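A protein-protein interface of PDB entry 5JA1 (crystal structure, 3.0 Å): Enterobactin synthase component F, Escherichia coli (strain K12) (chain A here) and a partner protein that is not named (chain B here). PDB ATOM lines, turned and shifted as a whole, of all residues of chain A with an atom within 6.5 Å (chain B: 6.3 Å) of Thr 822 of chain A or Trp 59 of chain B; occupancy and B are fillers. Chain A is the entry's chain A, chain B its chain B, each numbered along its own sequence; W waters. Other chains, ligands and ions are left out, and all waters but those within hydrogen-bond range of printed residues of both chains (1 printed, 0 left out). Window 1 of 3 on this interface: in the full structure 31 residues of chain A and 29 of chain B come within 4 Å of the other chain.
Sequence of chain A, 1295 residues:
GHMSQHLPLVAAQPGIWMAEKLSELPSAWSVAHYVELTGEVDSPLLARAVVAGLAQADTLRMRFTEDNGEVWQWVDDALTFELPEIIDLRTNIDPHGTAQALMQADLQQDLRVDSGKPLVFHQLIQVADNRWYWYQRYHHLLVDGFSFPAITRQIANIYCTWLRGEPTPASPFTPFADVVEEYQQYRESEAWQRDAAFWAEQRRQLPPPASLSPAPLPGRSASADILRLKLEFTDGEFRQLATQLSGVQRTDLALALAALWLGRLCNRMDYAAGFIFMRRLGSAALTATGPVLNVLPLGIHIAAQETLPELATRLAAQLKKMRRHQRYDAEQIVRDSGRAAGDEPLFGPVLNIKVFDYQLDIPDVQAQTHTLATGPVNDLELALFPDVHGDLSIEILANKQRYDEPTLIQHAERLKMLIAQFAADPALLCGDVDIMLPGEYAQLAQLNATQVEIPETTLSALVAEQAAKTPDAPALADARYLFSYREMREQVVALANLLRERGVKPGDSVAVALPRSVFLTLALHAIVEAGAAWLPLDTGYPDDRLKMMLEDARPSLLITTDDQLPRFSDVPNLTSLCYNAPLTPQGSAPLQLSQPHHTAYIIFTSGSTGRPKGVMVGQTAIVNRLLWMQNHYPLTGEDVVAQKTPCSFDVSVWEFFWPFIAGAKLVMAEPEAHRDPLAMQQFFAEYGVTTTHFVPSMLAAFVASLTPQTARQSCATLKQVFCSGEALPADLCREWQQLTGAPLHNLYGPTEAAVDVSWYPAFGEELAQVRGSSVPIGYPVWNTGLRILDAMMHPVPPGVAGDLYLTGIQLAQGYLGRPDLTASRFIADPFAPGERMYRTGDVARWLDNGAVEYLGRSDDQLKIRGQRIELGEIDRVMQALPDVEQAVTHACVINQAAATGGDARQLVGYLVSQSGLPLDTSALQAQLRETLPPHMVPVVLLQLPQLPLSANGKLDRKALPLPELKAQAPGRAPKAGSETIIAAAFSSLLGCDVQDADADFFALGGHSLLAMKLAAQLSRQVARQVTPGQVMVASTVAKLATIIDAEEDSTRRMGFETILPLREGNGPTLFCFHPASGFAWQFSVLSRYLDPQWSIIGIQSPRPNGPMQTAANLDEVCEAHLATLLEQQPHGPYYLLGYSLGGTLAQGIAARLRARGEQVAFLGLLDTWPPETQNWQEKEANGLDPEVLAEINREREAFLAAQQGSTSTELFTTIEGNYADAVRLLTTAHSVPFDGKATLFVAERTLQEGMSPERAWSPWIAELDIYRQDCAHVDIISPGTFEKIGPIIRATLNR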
ATOM      1  N   GLN A 813      24.291  27.051   3.963  1.00  0.00           N
ATOM      2  CA  GLN A 813      23.493  26.041   3.282  1.00  0.00           C
ATOM      3  C   GLN A 813      24.145  24.666   3.375  1.00  0.00           C
ATOM      4  O   GLN A 813      23.452  23.646   3.281  1.00  0.00           O
ATOM      5  CB  GLN A 813      23.273  26.439   1.821  1.00  0.00           C
ATOM      6  CG  GLN A 813      22.374  27.654   1.642  1.00  0.00           C
ATOM      7  CD  GLN A 813      22.482  28.261   0.257  1.00  0.00           C
ATOM      8  OE1 GLN A 813      23.492  28.097  -0.426  1.00  0.00           O
ATOM      9  NE2 GLN A 813      21.438  28.969  -0.168  1.00  0.00           N
ATOM     10  N   GLY A 814      25.456  24.619   3.573  1.00  0.00           N
ATOM     11  CA  GLY A 814      26.194  23.383   3.672  1.00  0.00           C
ATOM     12  C   GLY A 814      27.490  23.486   2.905  1.00  0.00           C
ATOM     13  O   GLY A 814      27.875  24.555   2.433  1.00  0.00           O
ATOM     14  N   TYR A 815      28.174  22.353   2.782  1.00  0.00           N
ATOM     15  CA  TYR A 815      29.427  22.284   2.048  1.00  0.00           C
ATOM     16  C   TYR A 815      29.164  21.917   0.594  1.00  0.00           C
ATOM     17  O   TYR A 815      28.315  21.073   0.295  1.00  0.00           O
ATOM     18  CB  TYR A 815      30.377  21.271   2.688  1.00  0.00           C
ATOM     19  CG  TYR A 815      30.890  21.704   4.041  1.00  0.00           C
ATOM     20  CD1 TYR A 815      31.793  22.752   4.157  1.00  0.00           C
ATOM     21  CD2 TYR A 815      30.474  21.066   5.202  1.00  0.00           C
ATOM     22  CE1 TYR A 815      32.266  23.155   5.393  1.00  0.00           C
ATOM     23  CE2 TYR A 815      30.943  21.460   6.442  1.00  0.00           C
ATOM     24  CZ  TYR A 815      31.839  22.505   6.533  1.00  0.00           C
ATOM     25  OH  TYR A 815      32.309  22.901   7.765  1.00  0.00           O
ATOM     26  N   LEU A 816      29.898  22.563  -0.306  1.00  0.00           N
ATOM     27  CA  LEU A 816      29.710  22.382  -1.739  1.00  0.00           C
ATOM     28  C   LEU A 816      30.308  21.046  -2.170  1.00  0.00           C
ATOM     29  O   LEU A 816      31.517  20.829  -2.037  1.00  0.00           O
ATOM     30  CB  LEU A 816      30.350  23.546  -2.492  1.00  0.00           C
ATOM     31  CG  LEU A 816      30.407  23.534  -4.019  1.00  0.00           C
ATOM     32  CD1 LEU A 816      29.046  23.247  -4.610  1.00  0.00           C
ATOM     33  CD2 LEU A 816      30.927  24.870  -4.521  1.00  0.00           C
ATOM     34  N   ARG A 818      29.866  18.130  -0.824  1.00  0.00           N
ATOM     35  CA  ARG A 818      30.279  17.310   0.313  1.00  0.00           C
ATOM     36  C   ARG A 818      29.085  17.044   1.221  1.00  0.00           C
ATOM     37  O   ARG A 818      28.949  17.662   2.286  1.00  0.00           O
ATOM     38  CB  ARG A 818      31.412  17.990   1.081  1.00  0.00           C
ATOM     39  CG  ARG A 818      32.616  18.329   0.215  1.00  0.00           C
ATOM     40  CD  ARG A 818      33.342  17.067  -0.206  1.00  0.00           C
ATOM     41  NE  ARG A 818      34.095  16.503   0.909  1.00  0.00           N
ATOM     42  CZ  ARG A 818      34.531  15.251   0.966  1.00  0.00           C
ATOM     43  NH1 ARG A 818      35.211  14.836   2.027  1.00  0.00           N
ATOM     44  NH2 ARG A 818      34.280  14.410  -0.028  1.00  0.00           N
ATOM     45  N   PRO A 819      28.200  16.120   0.835  1.00  0.00           N
ATOM     46  CA  PRO A 819      27.104  15.751   1.743  1.00  0.00           C
ATOM     47  C   PRO A 819      27.586  15.017   2.979  1.00  0.00           C
ATOM     48  O   PRO A 819      26.958  15.133   4.040  1.00  0.00           O
ATOM     49  CB  PRO A 819      26.208  14.865   0.870  1.00  0.00           C
ATOM     50  CG  PRO A 819      27.138  14.287  -0.137  1.00  0.00           C
ATOM     51  CD  PRO A 819      28.150  15.361  -0.425  1.00  0.00           C
ATOM     52  N   ASP A 820      28.685  14.266   2.879  1.00  0.00           N
ATOM     53  CA  ASP A 820      29.215  13.575   4.048  1.00  0.00           C
ATOM     54  C   ASP A 820      29.710  14.564   5.096  1.00  0.00           C
ATOM     55  O   ASP A 820      29.464  14.385   6.294  1.00  0.00           O
ATOM     56  CB  ASP A 820      30.333  12.618   3.631  1.00  0.00           C
ATOM     57  CG  ASP A 820      31.400  13.298   2.794  1.00  0.00           C
ATOM     58  OD1 ASP A 820      31.095  14.330   2.161  1.00  0.00           O
ATOM     59  OD2 ASP A 820      32.545  12.798   2.765  1.00  0.00           O
ATOM     60  N   LEU A 821      30.404  15.621   4.664  1.00  0.00           N
ATOM     61  CA  LEU A 821      30.851  16.641   5.607  1.00  0.00           C
ATOM     62  C   LEU A 821      29.672  17.408   6.191  1.00  0.00           C
ATOM     63  O   LEU A 821      29.645  17.695   7.393  1.00  0.00           O
ATOM     64  CB  LEU A 821      31.821  17.604   4.924  1.00  0.00           C
ATOM     65  CG  LEU A 821      33.146  17.037   4.416  1.00  0.00           C
ATOM     66  CD1 LEU A 821      33.957  18.138   3.762  1.00  0.00           C
ATOM     67  CD2 LEU A 821      33.928  16.392   5.548  1.00  0.00           C
ATOM     68  N   THR A 822      28.690  17.751   5.351  1.00  0.00           N
ATOM     69  CA  THR A 822      27.535  18.513   5.815  1.00  0.00           C
ATOM     70  C   THR A 822      26.793  17.770   6.918  1.00  0.00           C
ATOM     71  O   THR A 822      26.526  18.329   7.989  1.00  0.00           O
ATOM     72  CB  THR A 822      26.596  18.801   4.645  1.00  0.00           C
ATOM     73  OG1 THR A 822      27.304  19.518   3.626  1.00  0.00           O
ATOM     74  CG2 THR A 822      25.409  19.632   5.108  1.00  0.00           C
ATOM     75  N   ALA A 823      26.459  16.500   6.676  1.00  0.00           N
ATOM     76  CA  ALA A 823      25.742  15.714   7.671  1.00  0.00           C
ATOM     77  C   ALA A 823      26.565  15.484   8.932  1.00  0.00           C
ATOM     78  O   ALA A 823      26.001  15.115   9.967  1.00  0.00           O
ATOM     79  CB  ALA A 823      25.316  14.372   7.072  1.00  0.00           C
ATOM     80  N   SER A 824      27.879  15.696   8.871  1.00  0.00           N
ATOM     81  CA  SER A 824      28.737  15.503  10.034  1.00  0.00           C
ATOM     82  C   SER A 824      28.885  16.771  10.868  1.00  0.00           C
ATOM     83  O   SER A 824      28.912  16.697  12.100  1.00  0.00           O
ATOM     84  CB  SER A 824      30.115  15.002   9.594  1.00  0.00           C
ATOM     85  OG  SER A 824      30.989  14.878  10.702  1.00  0.00           O
ATOM     86  N   ARG A 825      28.979  17.936  10.227  1.00  0.00           N
ATOM     87  CA  ARG A 825      29.132  19.202  10.937  1.00  0.00           C
ATOM     88  C   ARG A 825      27.809  19.935  11.149  1.00  0.00           C
ATOM     89  O   ARG A 825      27.622  20.571  12.190  1.00  0.00           O
ATOM     90  CB  ARG A 825      30.110  20.115  10.188  1.00  0.00           C
ATOM     91  CG  ARG A 825      31.477  19.493   9.888  1.00  0.00           C
ATOM     92  CD  ARG A 825      32.322  19.310  11.145  1.00  0.00           C
ATOM     93  NE  ARG A 825      32.847  20.571  11.665  1.00  0.00           N
ATOM     94  CZ  ARG A 825      33.649  20.667  12.722  1.00  0.00           C
ATOM     95  NH1 ARG A 825      34.026  19.578  13.378  1.00  0.00           N
ATOM     96  NH2 ARG A 825      34.078  21.855  13.127  1.00  0.00           N
ATOM     97  N   PHE A 826      26.885  19.860  10.189  1.00  0.00           N
ATOM     98  CA  PHE A 826      25.558  20.472  10.303  1.00  0.00           C
ATOM     99  C   PHE A 826      24.591  19.394  10.784  1.00  0.00           C
ATOM    100  O   PHE A 826      23.911  18.747   9.987  1.00  0.00           O
ATOM    101  CB  PHE A 826      25.100  21.063   8.972  1.00  0.00           C
ATOM    102  CG  PHE A 826      25.963  22.187   8.466  1.00  0.00           C
ATOM    103  CD1 PHE A 826      25.629  23.507   8.729  1.00  0.00           C
ATOM    104  CD2 PHE A 826      27.095  21.926   7.711  1.00  0.00           C
ATOM    105  CE1 PHE A 826      26.416  24.545   8.260  1.00  0.00           C
ATOM    106  CE2 PHE A 826      27.887  22.958   7.238  1.00  0.00           C
ATOM    107  CZ  PHE A 826      27.547  24.271   7.513  1.00  0.00           C
ATOM    108  N   ILE A 827      24.514  19.214  12.097  1.00  0.00           N
ATOM    109  CA  ILE A 827      23.802  18.089  12.675  1.00  0.00           C
ATOM    110  C   ILE A 827      22.407  18.518  13.111  1.00  0.00           C
ATOM    111  O   ILE A 827      22.044  19.690  13.061  1.00  0.00           O
ATOM    112  CB  ILE A 827      24.582  17.465  13.854  1.00  0.00           C
ATOM    113  CG1 ILE A 827      24.554  18.389  15.072  1.00  0.00           C
ATOM    114  CG2 ILE A 827      26.013  17.172  13.448  1.00  0.00           C
ATOM    115  CD1 ILE A 827      25.181  17.767  16.305  1.00  0.00           C
ATOM    116  N   ARG A 836      18.244  22.807  12.491  1.00  0.00           N
ATOM    117  CA  ARG A 836      19.610  22.340  12.323  1.00  0.00           C
ATOM    118  C   ARG A 836      20.545  23.145  13.218  1.00  0.00           C
ATOM    119  O   ARG A 836      20.200  24.223  13.709  1.00  0.00           O
ATOM    120  CB  ARG A 836      20.047  22.436  10.855  1.00  0.00           C
ATOM    121  CG  ARG A 836      20.943  21.302  10.401  1.00  0.00           C
ATOM    122  CD  ARG A 836      21.042  21.250   8.886  1.00  0.00           C
ATOM    123  NE  ARG A 836      21.341  22.556   8.309  1.00  0.00           N
ATOM    124  CZ  ARG A 836      21.791  22.736   7.073  1.00  0.00           C
ATOM    125  NH1 ARG A 836      22.004  21.689   6.288  1.00  0.00           N
ATOM    126  NH2 ARG A 836      22.037  23.960   6.625  1.00  0.00           N
ATOM    127  N   GLY B  24      14.445  17.813   3.540  1.00  0.00           N
ATOM    128  CA  GLY B  24      15.352  16.956   2.795  1.00  0.00           C
ATOM    129  C   GLY B  24      16.809  17.133   3.154  1.00  0.00           C
ATOM    130  O   GLY B  24      17.678  16.975   2.290  1.00  0.00           O
ATOM    131  N   GLN B  25      17.102  17.462   4.405  1.00  0.00           N
ATOM    132  CA  GLN B  25      18.473  17.612   4.868  1.00  0.00           C
ATOM    133  C   GLN B  25      18.865  16.401   5.704  1.00  0.00           C
ATOM    134  O   GLN B  25      18.041  15.828   6.422  1.00  0.00           O
ATOM    135  CB  GLN B  25      18.643  18.896   5.679  1.00  0.00           C
ATOM    136  CG  GLN B  25      18.507  20.164   4.850  1.00  0.00           C
ATOM    137  CD  GLN B  25      18.484  21.418   5.698  1.00  0.00           C
ATOM    138  OE1 GLN B  25      18.041  21.398   6.845  1.00  0.00           O
ATOM    139  NE2 GLN B  25      18.964  22.522   5.135  1.00  0.00           N
ATOM    140  N   PHE B  26      20.132  16.013   5.600  1.00  0.00           N
ATOM    141  CA  PHE B  26      20.633  14.803   6.233  1.00  0.00           C
ATOM    142  C   PHE B  26      21.579  15.149   7.373  1.00  0.00           C
ATOM    143  O   PHE B  26      22.434  16.029   7.245  1.00  0.00           O
ATOM    144  CB  PHE B  26      21.341  13.904   5.217  1.00  0.00           C
ATOM    145  CG  PHE B  26      20.409  13.267   4.230  1.00  0.00           C
ATOM    146  CD1 PHE B  26      19.694  12.132   4.570  1.00  0.00           C
ATOM    147  CD2 PHE B  26      20.241  13.808   2.969  1.00  0.00           C
ATOM    148  CE1 PHE B  26      18.831  11.547   3.667  1.00  0.00           C
ATOM    149  CE2 PHE B  26      19.381  13.225   2.061  1.00  0.00           C
ATOM    150  CZ  PHE B  26      18.675  12.093   2.412  1.00  0.00           C
ATOM    151  N   SER B  27      21.411  14.446   8.488  1.00  0.00           N
ATOM    152  CA  SER B  27      22.242  14.609   9.668  1.00  0.00           C
ATOM    153  C   SER B  27      22.635  13.241  10.201  1.00  0.00           C
ATOM    154  O   SER B  27      21.800  12.336  10.288  1.00  0.00           O
ATOM    155  CB  SER B  27      21.509  15.395  10.760  1.00  0.00           C
ATOM    156  OG  SER B  27      22.222  15.348  11.984  1.00  0.00           O
ATOM    157  N   TRP B  54      27.126   6.246   1.673  1.00  0.00           N
ATOM    158  CA  TRP B  54      25.692   6.386   1.443  1.00  0.00           C
ATOM    159  C   TRP B  54      25.321   7.829   1.125  1.00  0.00           C
ATOM    160  O   TRP B  54      24.515   8.084   0.222  1.00  0.00           O
ATOM    161  CB  TRP B  54      24.917   5.890   2.666  1.00  0.00           C
ATOM    162  CG  TRP B  54      23.432   5.832   2.461  1.00  0.00           C
ATOM    163  CD1 TRP B  54      22.698   4.740   2.105  1.00  0.00           C
ATOM    164  CD2 TRP B  54      22.501   6.913   2.603  1.00  0.00           C
ATOM    165  NE1 TRP B  54      21.369   5.071   2.015  1.00  0.00           N
ATOM    166  CE2 TRP B  54      21.220   6.400   2.315  1.00  0.00           C
ATOM    167  CE3 TRP B  54      22.623   8.264   2.944  1.00  0.00           C
ATOM    168  CZ2 TRP B  54      20.073   7.189   2.356  1.00  0.00           C
ATOM    169  CZ3 TRP B  54      21.483   9.046   2.985  1.00  0.00           C
ATOM    170  CH2 TRP B  54      20.225   8.505   2.694  1.00  0.00           C
ATOM    171  N   LEU B  55      25.898   8.784   1.859  1.00  0.00           N
ATOM    172  CA  LEU B  55      25.525  10.185   1.687  1.00  0.00           C
ATOM    173  C   LEU B  55      25.947  10.715   0.321  1.00  0.00           C
ATOM    174  O   LEU B  55      25.228  11.512  -0.289  1.00  0.00           O
ATOM    175  CB  LEU B  55      26.138  11.027   2.807  1.00  0.00           C
ATOM    176  CG  LEU B  55      25.465  10.903   4.174  1.00  0.00           C
ATOM    177  CD1 LEU B  55      26.419  11.308   5.285  1.00  0.00           C
ATOM    178  CD2 LEU B  55      24.212  11.758   4.211  1.00  0.00           C
ATOM    179  N   GLU B  56      27.104  10.278  -0.179  1.00  0.00           N
ATOM    180  CA  GLU B  56      27.570  10.749  -1.479  1.00  0.00           C
ATOM    181  C   GLU B  56      26.720  10.224  -2.630  1.00  0.00           C
ATOM    182  O   GLU B  56      26.809  10.760  -3.740  1.00  0.00           O
ATOM    183  CB  GLU B  56      29.035  10.359  -1.685  1.00  0.00           C
ATOM    184  CG  GLU B  56      30.009  11.182  -0.856  1.00  0.00           C
ATOM    185  CD  GLU B  56      31.447  10.717  -0.996  1.00  0.00           C
ATOM    186  OE1 GLU B  56      31.670   9.637  -1.581  1.00  0.00           O
ATOM    187  OE2 GLU B  56      32.354  11.435  -0.519  1.00  0.00           O
ATOM    188  N   ALA B  57      25.894   9.203  -2.393  1.00  0.00           N
ATOM    189  CA  ALA B  57      25.057   8.625  -3.434  1.00  0.00           C
ATOM    190  C   ALA B  57      23.581   8.973  -3.303  1.00  0.00           C
ATOM    191  O   ALA B  57      22.816   8.693  -4.232  1.00  0.00           O
ATOM    192  CB  ALA B  57      25.211   7.097  -3.454  1.00  0.00           C
ATOM    193  N   HIS B  58      23.157   9.569  -2.188  1.00  0.00           N
ATOM    194  CA  HIS B  58      21.748   9.867  -1.964  1.00  0.00           C
ATOM    195  C   HIS B  58      21.462  11.335  -1.680  1.00  0.00           C
ATOM    196  O   HIS B  58      20.290  11.700  -1.526  1.00  0.00           O
ATOM    197  CB  HIS B  58      21.200   9.011  -0.813  1.00  0.00           C
ATOM    198  CG  HIS B  58      20.977   7.578  -1.180  1.00  0.00           C
ATOM    199  ND1 HIS B  58      22.011   6.686  -1.365  1.00  0.00           N
ATOM    200  CD2 HIS B  58      19.837   6.883  -1.407  1.00  0.00           C
ATOM    201  CE1 HIS B  58      21.518   5.503  -1.684  1.00  0.00           C
ATOM    202  NE2 HIS B  58      20.201   5.596  -1.717  1.00  0.00           N
ATOM    203  N   TRP B  59      22.484  12.189  -1.606  1.00  0.00           N
ATOM    204  CA  TRP B  59      22.288  13.622  -1.365  1.00  0.00           C
ATOM    205  C   TRP B  59      23.222  14.381  -2.305  1.00  0.00           C
ATOM    206  O   TRP B  59      24.353  14.714  -1.940  1.00  0.00           O
ATOM    207  CB  TRP B  59      22.540  13.985   0.092  1.00  0.00           C
ATOM    208  CG  TRP B  59      22.013  15.338   0.462  1.00  0.00           C
ATOM    209  CD1 TRP B  59      21.147  16.108  -0.260  1.00  0.00           C
ATOM    210  CD2 TRP B  59      22.319  16.086   1.646  1.00  0.00           C
ATOM    211  NE1 TRP B  59      20.894  17.285   0.401  1.00  0.00           N
ATOM    212  CE2 TRP B  59      21.602  17.296   1.574  1.00  0.00           C
ATOM    213  CE3 TRP B  59      23.131  15.847   2.761  1.00  0.00           C
ATOM    214  CZ2 TRP B  59      21.671  18.267   2.574  1.00  0.00           C
ATOM    215  CZ3 TRP B  59      23.198  16.812   3.752  1.00  0.00           C
ATOM    216  CH2 TRP B  59      22.473  18.006   3.652  1.00  0.00           C
ATOM    217  N   ARG B  60      22.735  14.655  -3.515  1.00  0.00           N
ATOM    218  CA  ARG B  60      23.511  15.361  -4.529  1.00  0.00           C
ATOM    219  C   ARG B  60      22.870  16.679  -4.946  1.00  0.00           C
ATOM    220  O   ARG B  60      23.263  17.253  -5.969  1.00  0.00           O
ATOM    221  CB  ARG B  60      23.720  14.466  -5.754  1.00  0.00           C
ATOM    222  CG  ARG B  60      24.535  13.215  -5.467  1.00  0.00           C
ATOM    223  CD  ARG B  60      24.630  12.326  -6.697  1.00  0.00           C
ATOM    224  NE  ARG B  60      25.541  11.203  -6.491  1.00  0.00           N
ATOM    225  CZ  ARG B  60      26.828  11.216  -6.824  1.00  0.00           C
ATOM    226  NH1 ARG B  60      27.360  12.295  -7.381  1.00  0.00           N
ATOM    227  NH2 ARG B  60      27.585  10.150  -6.600  1.00  0.00           N
ATOM    228  N   THR B  61      21.889  17.173  -4.186  1.00  0.00           N
ATOM    229  CA  THR B  61      21.263  18.466  -4.442  1.00  0.00           C
ATOM    230  C   THR B  61      21.941  19.600  -3.683  1.00  0.00           C
ATOM    231  O   THR B  61      21.299  20.617  -3.388  1.00  0.00           O
ATOM    232  CB  THR B  61      19.776  18.410  -4.086  1.00  0.00           C
ATOM    233  OG1 THR B  61      19.628  18.126  -2.689  1.00  0.00           O
ATOM    234  CG2 THR B  61      19.072  17.329  -4.890  1.00  0.00           C
ATOM    235  N   LEU B  62      23.227  19.458  -3.371  1.00  0.00           N
ATOM    236  CA  LEU B  62      23.933  20.363  -2.465  1.00  0.00           C
ATOM    237  C   LEU B  62      24.811  21.363  -3.210  1.00  0.00           C
ATOM    238  O   LEU B  62      25.894  21.716  -2.736  1.00  0.00           O
ATOM    239  CB  LEU B  62      24.761  19.552  -1.472  1.00  0.00           C
ATOM    240  CG  LEU B  62      25.078  20.145  -0.099  1.00  0.00           C
ATOM    241  CD1 LEU B  62      23.832  20.735   0.537  1.00  0.00           C
ATOM    242  CD2 LEU B  62      25.676  19.074   0.797  1.00  0.00           C
HETATM  243  O   HOH W   1      22.723  18.672   7.378  1.00  0.00           O
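The side-chain hydroxyl of Thr 822 of chain A is in hydrogen-bond range of the backbone NH of Tyr 815 of chain A (3.1 Å).
The indole nitrogen of Trp 59 of chain B sits at hydrogen-bond distance from the side-chain hydroxyl of Thr 61 of chain B, at 3.4 Å.
OD2 of Asp 820 of chain A is in salt-bridge range of NH1 of Arg 818 of chain A (3.4 Å).
The guanidinium group of Arg 60 of chain B is in hydrogen-bond range of the backbone carbonyl oxygen of Glu 56 of chain B.
O of Arg 818 of chain A lies within hydrogen-bond range of OG1 of Thr 822 of chain A, 2.8 Å away.
Of the 15 printed residues of chain A, 9 touch a printed residue of chain B.
Of the 13 printed residues of chain B, 7 touch a printed residue of chain A.
Hydrophobic or aromatic side chains of chain B that line the printed part of chain A: Leu 55, Trp 59 and Leu 62.
Water W1 lies within hydrogen-bond range of O of Phe 26 of chain B, O of Phe 826 of chain A and NH1 of Arg 836 of chain A.
NE2 of Gln 25 of chain B lies close to NH1 of Arg 836 of chain A, 3.4 Å away.
NH2 of Arg 818 of chain A is in salt-bridge range of OE2 of Glu 56 of chain B, at 3.6 Å.
Among the printed residues, pairs that only touch across the chains: Tyr 815 of chain A with Leu 62 of chain B, Leu 816 of chain A with Leu 62 of chain B, Arg 818 of chain A with Leu 62 of chain B, Pro 819 of chain A with Leu 55 of chain B, Pro 819 of chain A with Glu 56 of chain B, Pro 819 of chain A with Trp 59 of chain B, Pro 819 of chain A with Leu 62 of chain B, Asp 820 of chain A with Leu 55 of chain B, Asp 820 of chain A with Glu 56 of chain B, Thr 822 of chain A with Trp 59 of chain B, Thr 822 of chain A with Leu 62 of chain B, Ala 823 of chain A with Phe 26 of chain B, Ala 823 of chain A with Ser 27 of chain B, Ala 823 of chain A with Leu 55 of chain B and Ile 827 of chain A with Ser 27 of chain B.
Thr 822 of chain A touches two residues of chain B.
Of chain A, only Pro 819 (3.3 Å) and Thr 822 (3.7 Å) come within 4 Å of Trp 59 of chain B.
Of the printed residues of chain A, Leu 62 of chain B touches Tyr 815 (3.3 Å), Leu 816 (3.97 Å), Arg 818 (3.9 Å), Pro 819 (3.7 Å) and Thr 822 (3.3 Å).
Of the printed residues of chain A, Phe 26 of chain B touches Ala 823.
Of the printed residues of chain A, Glu 56 of chain B touches Arg 818, Pro 819 and Asp 820.
Of the printed residues of chain B, Pro 819 of chain A touches Leu 55, Glu 56, Trp 59 and Leu 62.
Of the printed residues of chain B, Tyr 815 of chain A touches Leu 62.
The nearest printed residue of chain A that does not touch Leu 55 of chain B is Ser 824 of chain A (5.9 Å).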
